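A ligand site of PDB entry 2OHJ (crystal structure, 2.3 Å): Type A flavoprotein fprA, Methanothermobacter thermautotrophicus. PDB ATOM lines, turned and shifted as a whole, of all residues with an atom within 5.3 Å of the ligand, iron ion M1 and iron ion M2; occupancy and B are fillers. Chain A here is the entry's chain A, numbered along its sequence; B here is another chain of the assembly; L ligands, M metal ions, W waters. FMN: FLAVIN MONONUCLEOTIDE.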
ATOM      1  N   ASP A 264     -26.784  -9.791  17.494  1.00  0.00           N
ATOM      2  CA  ASP A 264     -27.228  -8.407  17.503  1.00  0.00           C
ATOM      3  C   ASP A 264     -26.989  -7.859  16.092  1.00  0.00           C
ATOM      4  O   ASP A 264     -26.321  -8.494  15.283  1.00  0.00           O
ATOM      5  CB  ASP A 264     -26.491  -7.579  18.555  1.00  0.00           C
ATOM      6  CG  ASP A 264     -27.404  -6.521  19.234  1.00  0.00           C
ATOM      7  OD1 ASP A 264     -28.295  -5.965  18.556  1.00  0.00           O
ATOM      8  OD2 ASP A 264     -27.233  -6.263  20.454  1.00  0.00           O
ATOM      9  N   THR A 265     -27.552  -6.688  15.802  1.00  0.00           N
ATOM     10  CA  THR A 265     -27.454  -6.080  14.483  1.00  0.00           C
ATOM     11  C   THR A 265     -27.738  -4.581  14.624  1.00  0.00           C
ATOM     12  O   THR A 265     -28.371  -4.156  15.600  1.00  0.00           O
ATOM     13  CB  THR A 265     -28.457  -6.732  13.495  1.00  0.00           C
ATOM     14  OG1 THR A 265     -28.156  -6.323  12.159  1.00  0.00           O
ATOM     15  CG2 THR A 265     -29.912  -6.378  13.842  1.00  0.00           C
ATOM     16  N   MET A 266     -27.247  -3.799  13.668  1.00  0.00           N
ATOM     17  CA  MET A 266     -27.532  -2.364  13.602  1.00  0.00           C
ATOM     18  C   MET A 266     -28.375  -2.082  12.378  1.00  0.00           C
ATOM     19  O   MET A 266     -29.392  -1.406  12.462  1.00  0.00           O
ATOM     20  CB  MET A 266     -26.234  -1.541  13.565  1.00  0.00           C
ATOM     21  CG  MET A 266     -25.313  -1.731  14.757  1.00  0.00           C
ATOM     22  SD  MET A 266     -23.810  -0.722  14.624  1.00  0.00           S
ATOM     23  CE  MET A 266     -22.863  -1.592  13.352  1.00  0.00           C
ATOM     24  N   HIS A 267     -27.961  -2.628  11.230  1.00  0.00           N
ATOM     25  CA  HIS A 267     -28.673  -2.392   9.988  1.00  0.00           C
ATOM     26  C   HIS A 267     -29.453  -3.615   9.474  1.00  0.00           C
ATOM     27  O   HIS A 267     -30.000  -3.549   8.365  1.00  0.00           O
ATOM     28  CB  HIS A 267     -27.724  -1.898   8.873  1.00  0.00           C
ATOM     29  CG  HIS A 267     -26.951  -0.656   9.207  1.00  0.00           C
ATOM     30  ND1 HIS A 267     -25.720  -0.374   8.647  1.00  0.00           N
ATOM     31  CD2 HIS A 267     -27.224   0.380  10.040  1.00  0.00           C
ATOM     32  CE1 HIS A 267     -25.273   0.769   9.115  1.00  0.00           C
ATOM     33  NE2 HIS A 267     -26.165   1.252   9.969  1.00  0.00           N
ATOM     34  N   GLY A 268     -29.483  -4.723  10.227  1.00  0.00           N
ATOM     35  CA  GLY A 268     -30.204  -5.923   9.811  1.00  0.00           C
ATOM     36  C   GLY A 268     -29.527  -7.027   8.991  1.00  0.00           C
ATOM     37  O   GLY A 268     -30.146  -8.056   8.738  1.00  0.00           O
ATOM     38  N   SER A 269     -28.292  -6.827   8.538  1.00  0.00           N
ATOM     39  CA  SER A 269     -27.564  -7.838   7.761  1.00  0.00           C
ATOM     40  C   SER A 269     -27.234  -9.093   8.555  1.00  0.00           C
ATOM     41  O   SER A 269     -27.333 -10.202   8.025  1.00  0.00           O
ATOM     42  CB  SER A 269     -26.257  -7.273   7.195  1.00  0.00           C
ATOM     43  OG  SER A 269     -26.502  -6.366   6.157  1.00  0.00           O
ATOM     44  N   THR A 270     -26.780  -8.906   9.795  1.00  0.00           N
ATOM     45  CA  THR A 270     -26.508 -10.001  10.707  1.00  0.00           C
ATOM     46  C   THR A 270     -27.802 -10.726  11.100  1.00  0.00           C
ATOM     47  O   THR A 270     -27.782 -11.916  11.324  1.00  0.00           O
ATOM     48  CB  THR A 270     -25.734  -9.515  11.961  1.00  0.00           C
ATOM     49  OG1 THR A 270     -24.567  -8.815  11.516  1.00  0.00           O
ATOM     50  CG2 THR A 270     -25.296 -10.676  12.826  1.00  0.00           C
ATOM     51  N   ARG A 271     -28.912  -9.993  11.143  1.00  0.00           N
ATOM     52  CA  ARG A 271     -30.218 -10.604  11.338  1.00  0.00           C
ATOM     53  C   ARG A 271     -30.625 -11.520  10.172  1.00  0.00           C
ATOM     54  O   ARG A 271     -31.063 -12.633  10.381  1.00  0.00           O
ATOM     55  CB  ARG A 271     -31.275  -9.535  11.614  1.00  0.00           C
ATOM     56  CG  ARG A 271     -32.674 -10.092  11.667  1.00  0.00           C
ATOM     57  CD  ARG A 271     -33.697  -9.135  12.262  1.00  0.00           C
ATOM     58  NE  ARG A 271     -33.487  -7.746  11.877  1.00  0.00           N
ATOM     59  CZ  ARG A 271     -33.274  -6.770  12.752  1.00  0.00           C
ATOM     60  NH1 ARG A 271     -33.235  -7.035  14.065  1.00  0.00           N
ATOM     61  NH2 ARG A 271     -33.087  -5.532  12.320  1.00  0.00           N
ATOM     62  N   PRO A 316     -22.390  -7.516  14.099  1.00  0.00           N
ATOM     63  CA  PRO A 316     -21.619  -6.622  13.254  1.00  0.00           C
ATOM     64  C   PRO A 316     -20.310  -6.186  13.939  1.00  0.00           C
ATOM     65  O   PRO A 316     -20.145  -6.368  15.153  1.00  0.00           O
ATOM     66  CB  PRO A 316     -22.552  -5.425  13.066  1.00  0.00           C
ATOM     67  CG  PRO A 316     -23.433  -5.415  14.232  1.00  0.00           C
ATOM     68  CD  PRO A 316     -23.618  -6.868  14.603  1.00  0.00           C
ATOM     69  N   THR A 317     -19.405  -5.631  13.143  1.00  0.00           N
ATOM     70  CA  THR A 317     -18.130  -5.132  13.648  1.00  0.00           C
ATOM     71  C   THR A 317     -18.228  -3.637  13.813  1.00  0.00           C
ATOM     72  O   THR A 317     -18.730  -2.955  12.922  1.00  0.00           O
ATOM     73  CB  THR A 317     -16.967  -5.488  12.680  1.00  0.00           C
ATOM     74  OG1 THR A 317     -16.838  -6.917  12.614  1.00  0.00           O
ATOM     75  CG2 THR A 317     -15.644  -4.873  13.141  1.00  0.00           C
ATOM     76  N   ILE A 318     -17.787  -3.156  14.970  1.00  0.00           N
ATOM     77  CA  ILE A 318     -17.581  -1.720  15.177  1.00  0.00           C
ATOM     78  C   ILE A 318     -16.174  -1.465  15.705  1.00  0.00           C
ATOM     79  O   ILE A 318     -15.782  -1.988  16.757  1.00  0.00           O
ATOM     80  CB  ILE A 318     -18.735  -1.017  16.012  1.00  0.00           C
ATOM     81  CG1 ILE A 318     -18.155   0.026  16.971  1.00  0.00           C
ATOM     82  CG2 ILE A 318     -19.662  -2.002  16.706  1.00  0.00           C
ATOM     83  CD1 ILE A 318     -19.045   0.357  18.137  1.00  0.00           C
ATOM     84  N   TYR A 319     -15.406  -0.707  14.937  1.00  0.00           N
ATOM     85  CA  TYR A 319     -14.008  -0.412  15.230  1.00  0.00           C
ATOM     86  C   TYR A 319     -13.220  -1.648  15.713  1.00  0.00           C
ATOM     87  O   TYR A 319     -12.606  -1.635  16.782  1.00  0.00           O
ATOM     88  CB  TYR A 319     -13.896   0.763  16.206  1.00  0.00           C
ATOM     89  CG  TYR A 319     -14.489   2.040  15.654  1.00  0.00           C
ATOM     90  CD1 TYR A 319     -14.142   2.505  14.378  1.00  0.00           C
ATOM     91  CD2 TYR A 319     -15.412   2.793  16.393  1.00  0.00           C
ATOM     92  CE1 TYR A 319     -14.684   3.677  13.864  1.00  0.00           C
ATOM     93  CE2 TYR A 319     -15.959   3.964  15.888  1.00  0.00           C
ATOM     94  CZ  TYR A 319     -15.597   4.406  14.628  1.00  0.00           C
ATOM     95  OH  TYR A 319     -16.135   5.556  14.115  1.00  0.00           O
ATOM     96  N   ASP A 320     -13.262  -2.708  14.891  1.00  0.00           N
ATOM     97  CA  ASP A 320     -12.509  -3.953  15.133  1.00  0.00           C
ATOM     98  C   ASP A 320     -13.104  -4.945  16.101  1.00  0.00           C
ATOM     99  O   ASP A 320     -12.585  -6.060  16.217  1.00  0.00           O
ATOM    100  CB  ASP A 320     -11.066  -3.660  15.559  1.00  0.00           C
ATOM    101  CG  ASP A 320     -10.366  -2.813  14.575  1.00  0.00           C
ATOM    102  OD1 ASP A 320     -10.366  -3.166  13.375  1.00  0.00           O
ATOM    103  OD2 ASP A 320      -9.846  -1.769  15.004  1.00  0.00           O
ATOM    104  N   SER A 351     -21.780  -9.505   9.738  1.00  0.00           N
ATOM    105  CA  SER A 351     -21.578  -8.589   8.640  1.00  0.00           C
ATOM    106  C   SER A 351     -20.602  -7.500   9.060  1.00  0.00           C
ATOM    107  O   SER A 351     -20.561  -7.102  10.217  1.00  0.00           O
ATOM    108  CB  SER A 351     -22.919  -7.979   8.238  1.00  0.00           C
ATOM    109  OG  SER A 351     -22.798  -7.202   7.067  1.00  0.00           O
ATOM    110  N   MET A 352     -19.793  -7.026   8.121  1.00  0.00           N
ATOM    111  CA  MET A 352     -18.805  -5.994   8.408  1.00  0.00           C
ATOM    112  C   MET A 352     -18.699  -5.037   7.222  1.00  0.00           C
ATOM    113  O   MET A 352     -19.230  -5.311   6.161  1.00  0.00           O
ATOM    114  CB  MET A 352     -17.445  -6.600   8.820  1.00  0.00           C
ATOM    115  CG  MET A 352     -16.914  -7.748   7.936  1.00  0.00           C
ATOM    116  SD  MET A 352     -16.106  -7.125   6.452  1.00  0.00           S
ATOM    117  CE  MET A 352     -15.183  -8.546   5.847  1.00  0.00           C
ATOM    118  N   GLY A 353     -18.018  -3.912   7.413  1.00  0.00           N
ATOM    119  CA  GLY A 353     -17.936  -2.885   6.388  1.00  0.00           C
ATOM    120  C   GLY A 353     -16.550  -2.618   5.847  1.00  0.00           C
ATOM    121  O   GLY A 353     -16.374  -1.766   4.954  1.00  0.00           O
ATOM    122  N   GLY A 354     -15.560  -3.326   6.371  1.00  0.00           N
ATOM    123  CA  GLY A 354     -14.179  -3.143   5.955  1.00  0.00           C
ATOM    124  C   GLY A 354     -13.300  -4.309   6.343  1.00  0.00           C
ATOM    125  O   GLY A 354     -13.308  -5.344   5.685  1.00  0.00           O
ATOM    126  N   ASN A 355     -12.561  -4.162   7.440  1.00  0.00           N
ATOM    127  CA  ASN A 355     -11.586  -5.164   7.855  1.00  0.00           C
ATOM    128  C   ASN A 355     -12.163  -6.261   8.733  1.00  0.00           C
ATOM    129  O   ASN A 355     -11.549  -7.328   8.889  1.00  0.00           O
ATOM    130  CB  ASN A 355     -10.399  -4.496   8.544  1.00  0.00           C
ATOM    131  CG  ASN A 355      -9.570  -3.652   7.600  1.00  0.00           C
ATOM    132  OD1 ASN A 355      -8.775  -2.811   8.023  1.00  0.00           O
ATOM    133  ND2 ASN A 355      -9.760  -3.872   6.296  1.00  0.00           N
ATOM    134  N   GLY A 356     -13.330  -6.015   9.311  1.00  0.00           N
ATOM    135  CA  GLY A 356     -13.974  -6.982  10.189  1.00  0.00           C
ATOM    136  C   GLY A 356     -13.254  -7.079  11.525  1.00  0.00           C
ATOM    137  O   GLY A 356     -12.631  -6.124  11.951  1.00  0.00           O
ATOM    138  N   TYR A 381     -21.181  -6.171   4.337  1.00  0.00           N
ATOM    139  CA  TYR A 381     -22.431  -5.433   4.246  1.00  0.00           C
ATOM    140  C   TYR A 381     -23.621  -6.381   4.068  1.00  0.00           C
ATOM    141  O   TYR A 381     -23.688  -7.414   4.731  1.00  0.00           O
ATOM    142  CB  TYR A 381     -22.339  -4.337   3.165  1.00  0.00           C
ATOM    143  CG  TYR A 381     -21.492  -3.133   3.565  1.00  0.00           C
ATOM    144  CD1 TYR A 381     -21.597  -2.555   4.832  1.00  0.00           C
ATOM    145  CD2 TYR A 381     -20.597  -2.552   2.665  1.00  0.00           C
ATOM    146  CE1 TYR A 381     -20.842  -1.450   5.191  1.00  0.00           C
ATOM    147  CE2 TYR A 381     -19.831  -1.454   3.017  1.00  0.00           C
ATOM    148  CZ  TYR A 381     -19.955  -0.904   4.285  1.00  0.00           C
ATOM    149  OH  TYR A 381     -19.208   0.203   4.628  1.00  0.00           O
ATOM    150  N   VAL A 382     -24.540  -6.030   3.181  1.00  0.00           N
ATOM    151  CA  VAL A 382     -25.734  -6.821   2.925  1.00  0.00           C
ATOM    152  C   VAL A 382     -25.390  -8.131   2.170  1.00  0.00           C
ATOM    153  O   VAL A 382     -24.709  -8.103   1.133  1.00  0.00           O
ATOM    154  CB  VAL A 382     -26.808  -5.978   2.159  1.00  0.00           C
ATOM    155  CG1 VAL A 382     -28.070  -6.802   1.844  1.00  0.00           C
ATOM    156  CG2 VAL A 382     -27.152  -4.685   2.945  1.00  0.00           C
ATOM    157  N   TYR B  25     -29.172   4.058  18.517  1.00  0.00           N
ATOM    158  CA  TYR B  25     -28.680   3.250  17.385  1.00  0.00           C
ATOM    159  C   TYR B  25     -27.179   3.347  17.277  1.00  0.00           C
ATOM    160  O   TYR B  25     -26.583   4.276  17.821  1.00  0.00           O
ATOM    161  CB  TYR B  25     -29.384   3.601  16.067  1.00  0.00           C
ATOM    162  CG  TYR B  25     -28.855   4.791  15.274  1.00  0.00           C
ATOM    163  CD1 TYR B  25     -28.941   4.788  13.893  1.00  0.00           C
ATOM    164  CD2 TYR B  25     -28.288   5.919  15.899  1.00  0.00           C
ATOM    165  CE1 TYR B  25     -28.490   5.849  13.140  1.00  0.00           C
ATOM    166  CE2 TYR B  25     -27.809   7.002  15.140  1.00  0.00           C
ATOM    167  CZ  TYR B  25     -27.913   6.956  13.758  1.00  0.00           C
ATOM    168  OH  TYR B  25     -27.477   7.980  12.961  1.00  0.00           O
ATOM    169  N   HIS B  26     -26.576   2.368  16.586  1.00  0.00           N
ATOM    170  CA  HIS B  26     -25.119   2.273  16.485  1.00  0.00           C
ATOM    171  C   HIS B  26     -24.426   2.111  17.847  1.00  0.00           C
ATOM    172  O   HIS B  26     -23.227   2.381  17.973  1.00  0.00           O
ATOM    173  CB  HIS B  26     -24.535   3.517  15.768  1.00  0.00           C
ATOM    174  CG  HIS B  26     -24.982   3.684  14.336  1.00  0.00           C
ATOM    175  ND1 HIS B  26     -25.183   4.911  13.760  1.00  0.00           N
ATOM    176  CD2 HIS B  26     -25.271   2.770  13.385  1.00  0.00           C
ATOM    177  CE1 HIS B  26     -25.556   4.758  12.506  1.00  0.00           C
ATOM    178  NE2 HIS B  26     -25.615   3.463  12.248  1.00  0.00           N
ATOM    179  N   GLU B  85     -22.869   4.799   4.349  1.00  0.00           N
ATOM    180  CA  GLU B  85     -23.725   4.544   5.528  1.00  0.00           C
ATOM    181  C   GLU B  85     -25.208   4.851   5.233  1.00  0.00           C
ATOM    182  O   GLU B  85     -25.535   5.934   4.727  1.00  0.00           O
ATOM    183  CB  GLU B  85     -23.207   5.328   6.748  1.00  0.00           C
ATOM    184  CG  GLU B  85     -24.252   5.811   7.740  1.00  0.00           C
ATOM    185  CD  GLU B  85     -24.654   4.736   8.750  1.00  0.00           C
ATOM    186  OE1 GLU B  85     -23.767   4.030   9.291  1.00  0.00           O
ATOM    187  OE2 GLU B  85     -25.875   4.624   9.027  1.00  0.00           O
ATOM    188  N   LYS B  86     -26.069   3.880   5.547  1.00  0.00           N
ATOM    189  CA  LYS B  86     -27.479   3.886   5.107  1.00  0.00           C
ATOM    190  C   LYS B  86     -28.278   5.115   5.532  1.00  0.00           C
ATOM    191  O   LYS B  86     -29.288   5.435   4.911  1.00  0.00           O
ATOM    192  CB  LYS B  86     -28.211   2.577   5.479  1.00  0.00           C
ATOM    193  CG  LYS B  86     -28.722   2.488   6.907  1.00  0.00           C
ATOM    194  CD  LYS B  86     -29.339   1.114   7.241  1.00  0.00           C
ATOM    195  CE  LYS B  86     -30.765   0.931   6.699  1.00  0.00           C
ATOM    196  NZ  LYS B  86     -31.318  -0.466   6.962  1.00  0.00           N
ATOM    197  N   ASP B  87     -27.867   5.814   6.582  1.00  0.00           N
ATOM    198  CA  ASP B  87     -28.622   7.003   6.892  1.00  0.00           C
ATOM    199  C   ASP B  87     -28.291   8.234   6.061  1.00  0.00           C
ATOM    200  O   ASP B  87     -28.987   9.239   6.128  1.00  0.00           O
ATOM    201  CB  ASP B  87     -28.824   7.240   8.408  1.00  0.00           C
ATOM    202  CG  ASP B  87     -27.568   7.443   9.159  1.00  0.00           C
ATOM    203  OD1 ASP B  87     -26.602   7.948   8.555  1.00  0.00           O
ATOM    204  OD2 ASP B  87     -27.536   7.154  10.366  1.00  0.00           O
ATOM    205  N   LEU B 150      -8.787   5.113   8.322  1.00  0.00           N
ATOM    206  CA  LEU B 150      -8.798   3.668   8.610  1.00  0.00           C
ATOM    207  C   LEU B 150     -10.201   3.026   8.443  1.00  0.00           C
ATOM    208  O   LEU B 150     -10.421   2.273   7.494  1.00  0.00           O
ATOM    209  CB  LEU B 150      -8.161   3.344   9.976  1.00  0.00           C
ATOM    210  CG  LEU B 150      -7.523   1.986  10.321  1.00  0.00           C
ATOM    211  CD1 LEU B 150      -6.857   1.247   9.134  1.00  0.00           C
ATOM    212  CD2 LEU B 150      -6.536   2.157  11.496  1.00  0.00           C
ATOM    213  N   HIS B 151     -11.139   3.352   9.329  1.00  0.00           N
ATOM    214  CA  HIS B 151     -12.397   2.615   9.415  1.00  0.00           C
ATOM    215  C   HIS B 151     -13.644   3.225   8.768  1.00  0.00           C
ATOM    216  O   HIS B 151     -14.733   2.636   8.859  1.00  0.00           O
ATOM    217  CB  HIS B 151     -12.685   2.186  10.868  1.00  0.00           C
ATOM    218  CG  HIS B 151     -11.743   1.141  11.363  1.00  0.00           C
ATOM    219  ND1 HIS B 151     -11.576  -0.075  10.731  1.00  0.00           N
ATOM    220  CD2 HIS B 151     -10.898   1.138  12.422  1.00  0.00           C
ATOM    221  CE1 HIS B 151     -10.671  -0.785  11.382  1.00  0.00           C
ATOM    222  NE2 HIS B 151     -10.240  -0.077  12.408  1.00  0.00           N
ATOM    223  N   LEU B 202     -17.518   8.009  18.439  1.00  0.00           N
ATOM    224  CA  LEU B 202     -17.280   7.748  17.005  1.00  0.00           C
ATOM    225  C   LEU B 202     -15.885   8.114  16.465  1.00  0.00           C
ATOM    226  O   LEU B 202     -15.440   7.549  15.476  1.00  0.00           O
ATOM    227  CB  LEU B 202     -18.407   8.381  16.163  1.00  0.00           C
ATOM    228  CG  LEU B 202     -19.823   7.888  16.559  1.00  0.00           C
ATOM    229  CD1 LEU B 202     -20.929   8.746  16.012  1.00  0.00           C
ATOM    230  CD2 LEU B 202     -20.041   6.418  16.142  1.00  0.00           C
ATOM    231  N   LYS B 337     -10.303   2.729  22.021  1.00  0.00           N
ATOM    232  CA  LYS B 337      -8.841   2.924  22.080  1.00  0.00           C
ATOM    233  C   LYS B 337      -8.469   4.321  22.588  1.00  0.00           C
ATOM    234  O   LYS B 337      -7.792   5.096  21.899  1.00  0.00           O
ATOM    235  CB  LYS B 337      -8.182   2.587  20.722  1.00  0.00           C
ATOM    236  CG  LYS B 337      -8.729   1.280  20.103  1.00  0.00           C
ATOM    237  CD  LYS B 337      -7.992   0.747  18.890  1.00  0.00           C
ATOM    238  CE  LYS B 337      -8.751  -0.461  18.288  1.00  0.00           C
ATOM    239  NZ  LYS B 337     -10.090  -0.031  17.716  1.00  0.00           N
ATOM    240  N   ARG B 340      -5.135   6.402  22.353  1.00  0.00           N
ATOM    241  CA  ARG B 340      -4.807   7.165  21.159  1.00  0.00           C
ATOM    242  C   ARG B 340      -4.900   8.683  21.383  1.00  0.00           C
ATOM    243  O   ARG B 340      -4.325   9.471  20.612  1.00  0.00           O
ATOM    244  CB  ARG B 340      -5.649   6.689  19.984  1.00  0.00           C
ATOM    245  CG  ARG B 340      -5.248   5.297  19.586  1.00  0.00           C
ATOM    246  CD  ARG B 340      -5.943   4.785  18.346  1.00  0.00           C
ATOM    247  NE  ARG B 340      -5.357   3.517  17.914  1.00  0.00           N
ATOM    248  CZ  ARG B 340      -5.773   2.802  16.872  1.00  0.00           C
ATOM    249  NH1 ARG B 340      -6.803   3.223  16.115  1.00  0.00           N
ATOM    250  NH2 ARG B 340      -5.145   1.683  16.562  1.00  0.00           N
HETATM  251  N1  FMN L   1     -16.945  -2.447   9.806  1.00  0.00           N
HETATM  252  C2  FMN L   1     -15.653  -2.957   9.803  1.00  0.00           C
HETATM  253  O2  FMN L   1     -15.343  -3.866   9.031  1.00  0.00           O
HETATM  254  N3  FMN L   1     -14.720  -2.461  10.677  1.00  0.00           N
HETATM  255  C4  FMN L   1     -15.052  -1.447  11.547  1.00  0.00           C
HETATM  256  O4  FMN L   1     -14.243  -1.094  12.405  1.00  0.00           O
HETATM  257  C4A FMN L   1     -16.337  -0.917  11.555  1.00  0.00           C
HETATM  258  N5  FMN L   1     -16.652   0.096  12.422  1.00  0.00           N
HETATM  259  C5A FMN L   1     -17.926   0.630  12.459  1.00  0.00           C
HETATM  260  C6  FMN L   1     -18.222   1.645  13.368  1.00  0.00           C
HETATM  261  C7  FMN L   1     -19.520   2.188  13.406  1.00  0.00           C
HETATM  262  C7M FMN L   1     -19.902   3.111  14.544  1.00  0.00           C
HETATM  263  C8  FMN L   1     -20.501   1.702  12.520  1.00  0.00           C
HETATM  264  C8M FMN L   1     -21.923   2.185  12.558  1.00  0.00           C
HETATM  265  C9  FMN L   1     -20.184   0.684  11.631  1.00  0.00           C
HETATM  266  C9A FMN L   1     -18.900   0.129  11.586  1.00  0.00           C
HETATM  267  N10 FMN L   1     -18.579  -0.888  10.689  1.00  0.00           N
HETATM  268  C10 FMN L   1     -17.294  -1.419  10.680  1.00  0.00           C
HETATM  269  C1' FMN L   1     -19.495  -1.193   9.537  1.00  0.00           C
HETATM  270  C2' FMN L   1     -20.495  -2.293   9.919  1.00  0.00           C
HETATM  271  O2' FMN L   1     -19.809  -3.349  10.568  1.00  0.00           O
HETATM  272  C3' FMN L   1     -21.254  -2.788   8.683  1.00  0.00           C
HETATM  273  O3' FMN L   1     -22.093  -1.739   8.238  1.00  0.00           O
HETATM  274  C4' FMN L   1     -22.099  -4.062   8.904  1.00  0.00           C
HETATM  275  O4' FMN L   1     -22.705  -4.481   7.693  1.00  0.00           O
HETATM  276  C5' FMN L   1     -23.204  -3.929   9.938  1.00  0.00           C
HETATM  277  O5' FMN L   1     -23.969  -5.123   9.958  1.00  0.00           O
HETATM  278  P   FMN L   1     -25.486  -5.133  10.478  1.00  0.00           P
HETATM  279  O1P FMN L   1     -26.389  -4.839   9.316  1.00  0.00           O
HETATM  280  O2P FMN L   1     -25.809  -6.474  11.059  1.00  0.00           O
HETATM  281  O3P FMN L   1     -25.654  -4.061  11.544  1.00  0.00           O
HETATM  282 FE    FE M   1      -9.066  -0.380  14.037  1.00  0.00          FE
HETATM  283 FE    FE M   2     -26.507   3.230  10.322  1.00  0.00          FE
HETATM  284  O   HOH W   1     -25.289  -4.097   6.901  1.00  0.00           O
HETATM  285  O   HOH W   2     -24.446  -1.712   6.537  1.00  0.00           O
HETATM  286  O   HOH W   3      -9.095   1.438  15.120  1.00  0.00           O
HETATM  287  O   HOH W   4     -15.065   0.135   8.414  1.00  0.00           O
HETATM  288  O   HOH W   5     -12.674  -1.219   8.206  1.00  0.00           O
HETATM  289  O   HOH W   6      -6.709  -0.617  13.916  1.00  0.00           O
HETATM  290  O   HOH W   7     -12.204  -3.642  11.438  1.00  0.00           O
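Water W3 lies within hydrogen-bond range of the guanidinium group of Arg 340 of chain B (3.1 Å) and the side-chain amino group of Lys 337 of chain B (3.1 Å). Water W1 bridges the side-chain hydroxyl (OG) of Ser 269 (2.7 Å) and an oxygen (O4') of the ligand (2.7 Å). Water W7 lies within hydrogen-bond range of O of Gly 356 (2.6 Å), OD1 of Asp 320 (2.7 Å) and N3 of the ligand (2.9 Å). Water W2 bridges a ring nitrogen (ND1) of His 267 and an oxygen (O3') of the ligand. Water W5 lies within hydrogen-bond range of ND1 of His 151 of chain B (3.0 Å), N of Asn 355 (3.0 Å) and N3 of the ligand (3.4 Å). Water W4 bridges O of His 151 of chain B (2.6 Å) and N3 of the ligand (3.5 Å).
Iron ion M2 is bound by the side-chain carboxylate of Glu 85 of chain B (2.0 Å), a ring nitrogen (NE2) of His 267 (2.0 Å) and a ring nitrogen (NE2) of His 26 of chain B (2.1 Å). Iron ion M2 has three donor atoms within binding distance.
NZ of Lys 337 of chain B touches iron ion M1, 3.8 Å away. Three residues have an atom within 4 Å of iron ion M1: Asp 320, His 151 of chain B and Lys 337 of chain B.
Within 4 Å of iron ion M2: His 267, His 26 of chain B and Glu 85 of chain B. The nearest printed residue that does not touch iron ion M2 is Asp 87 of chain B (4.1 Å).
Residues that only touch the ligand: Tyr 381, Ile 318, Pro 316, Met 352 and Leu 202 of chain B. Hydrophobic or aromatic side chains that line the ligand: Met 266, His 267, Pro 316, Ile 318, Tyr 319, Met 352, Tyr 381, His 26 of chain B, His 151 of chain B and Leu 202 of chain B. 21 residues have an atom within 4 Å of the ligand: Thr 265, Met 266, His 267, Gly 268, Ser 269, Thr 270, Pro 316, Thr 317, Ile 318, Tyr 319, Asp 320, Ser 351, Met 352, Gly 353, Gly 354, Asn 355, Gly 356, Tyr 381, His 26 of chain B, His 151 of chain B and Leu 202 of chain B.
N of Gly 268 is in hydrogen-bond range of OG1 of Thr 265. The backbone carbonyl oxygen (O) of Ser 351 sits at hydrogen-bond distance from the backbone NH (N) of Thr 317, 3.5 Å away. OG of Ser 269 sits at hydrogen-bond distance from O of Tyr 381. The side-chain hydroxyl of Tyr 319 lies within hydrogen-bond range of the backbone carbonyl oxygen of Leu 202 of chain B (2.5 Å). The side-chain hydroxyl (OG1) of Thr 270 lies within hydrogen-bond range of the backbone NH (N) of Ser 351. OD2 of Asp 320 lies close to NZ of Lys 337 of chain B, 3.2 Å away. The backbone carbonyl oxygen of Gly 353 sits at hydrogen-bond distance from the side-chain hydroxyl of Tyr 381 (3.5 Å). The backbone carbonyl oxygen (O) of Tyr 319 is in hydrogen-bond range of the side-chain amino group (NZ) of Lys 337 of chain B, 3.1 Å away.
N of Thr 270 lies within hydrogen-bond range of O2P of the ligand, 2.9 Å away. OG1 of Thr 265 lies within hydrogen-bond range of O2P of the ligand (2.6 Å). The backbone NH (N) of Tyr 319 lies within hydrogen-bond range of an oxygen (O4) of the ligand (2.8 Å). O1P of the ligand is in hydrogen-bond range of N of Ser 269, 2.9 Å away. N of Gly 356 sits at hydrogen-bond distance from O2 of the ligand. O of Thr 317 lies within hydrogen-bond range of O2' of the ligand. O3P of the ligand sits at hydrogen-bond distance from N of Met 266 (2.7 Å). A ring nitrogen (ND1) of His 151 of chain B is in hydrogen-bond range of an oxygen (O4) of the ligand (3.3 Å). N of His 267 is in hydrogen-bond range of O3P of the ligand (2.7 Å). N of Gly 268 lies within hydrogen-bond range of O1P of the ligand, 3.2 Å away. An oxygen (O4') of the ligand lies within hydrogen-bond range of the side-chain hydroxyl (OG) of Ser 351, 2.8 Å away. N of Asn 355 sits at hydrogen-bond distance from O2 of the ligand, 3.2 Å away. An oxygen (O2) of the ligand sits at hydrogen-bond distance from the backbone NH (N) of Gly 354 (2.7 Å). N of Gly 353 sits at hydrogen-bond distance from N1 of the ligand (3.0 Å). N of Thr 317 lies within hydrogen-bond range of O2' of the ligand, 3.5 Å away. An oxygen (O2P) of the ligand is in hydrogen-bond range of the side-chain hydroxyl (OG1) of Thr 270. An oxygen (O4) of the ligand is in hydrogen-bond range of the backbone NH (N) of Asp 320, at 3.1 Å.
Iron ion M1 is bound by the side-chain carboxylate (OD2) of Asp 320, at 1.9 Å. NE2 of His 151 of chain B is bound to iron ion M1, at 2.0 Å. Water W3 is bound to iron ion M1 (2.1 Å). Iron ion M1 is bound by water W6, at 2.4 Å.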
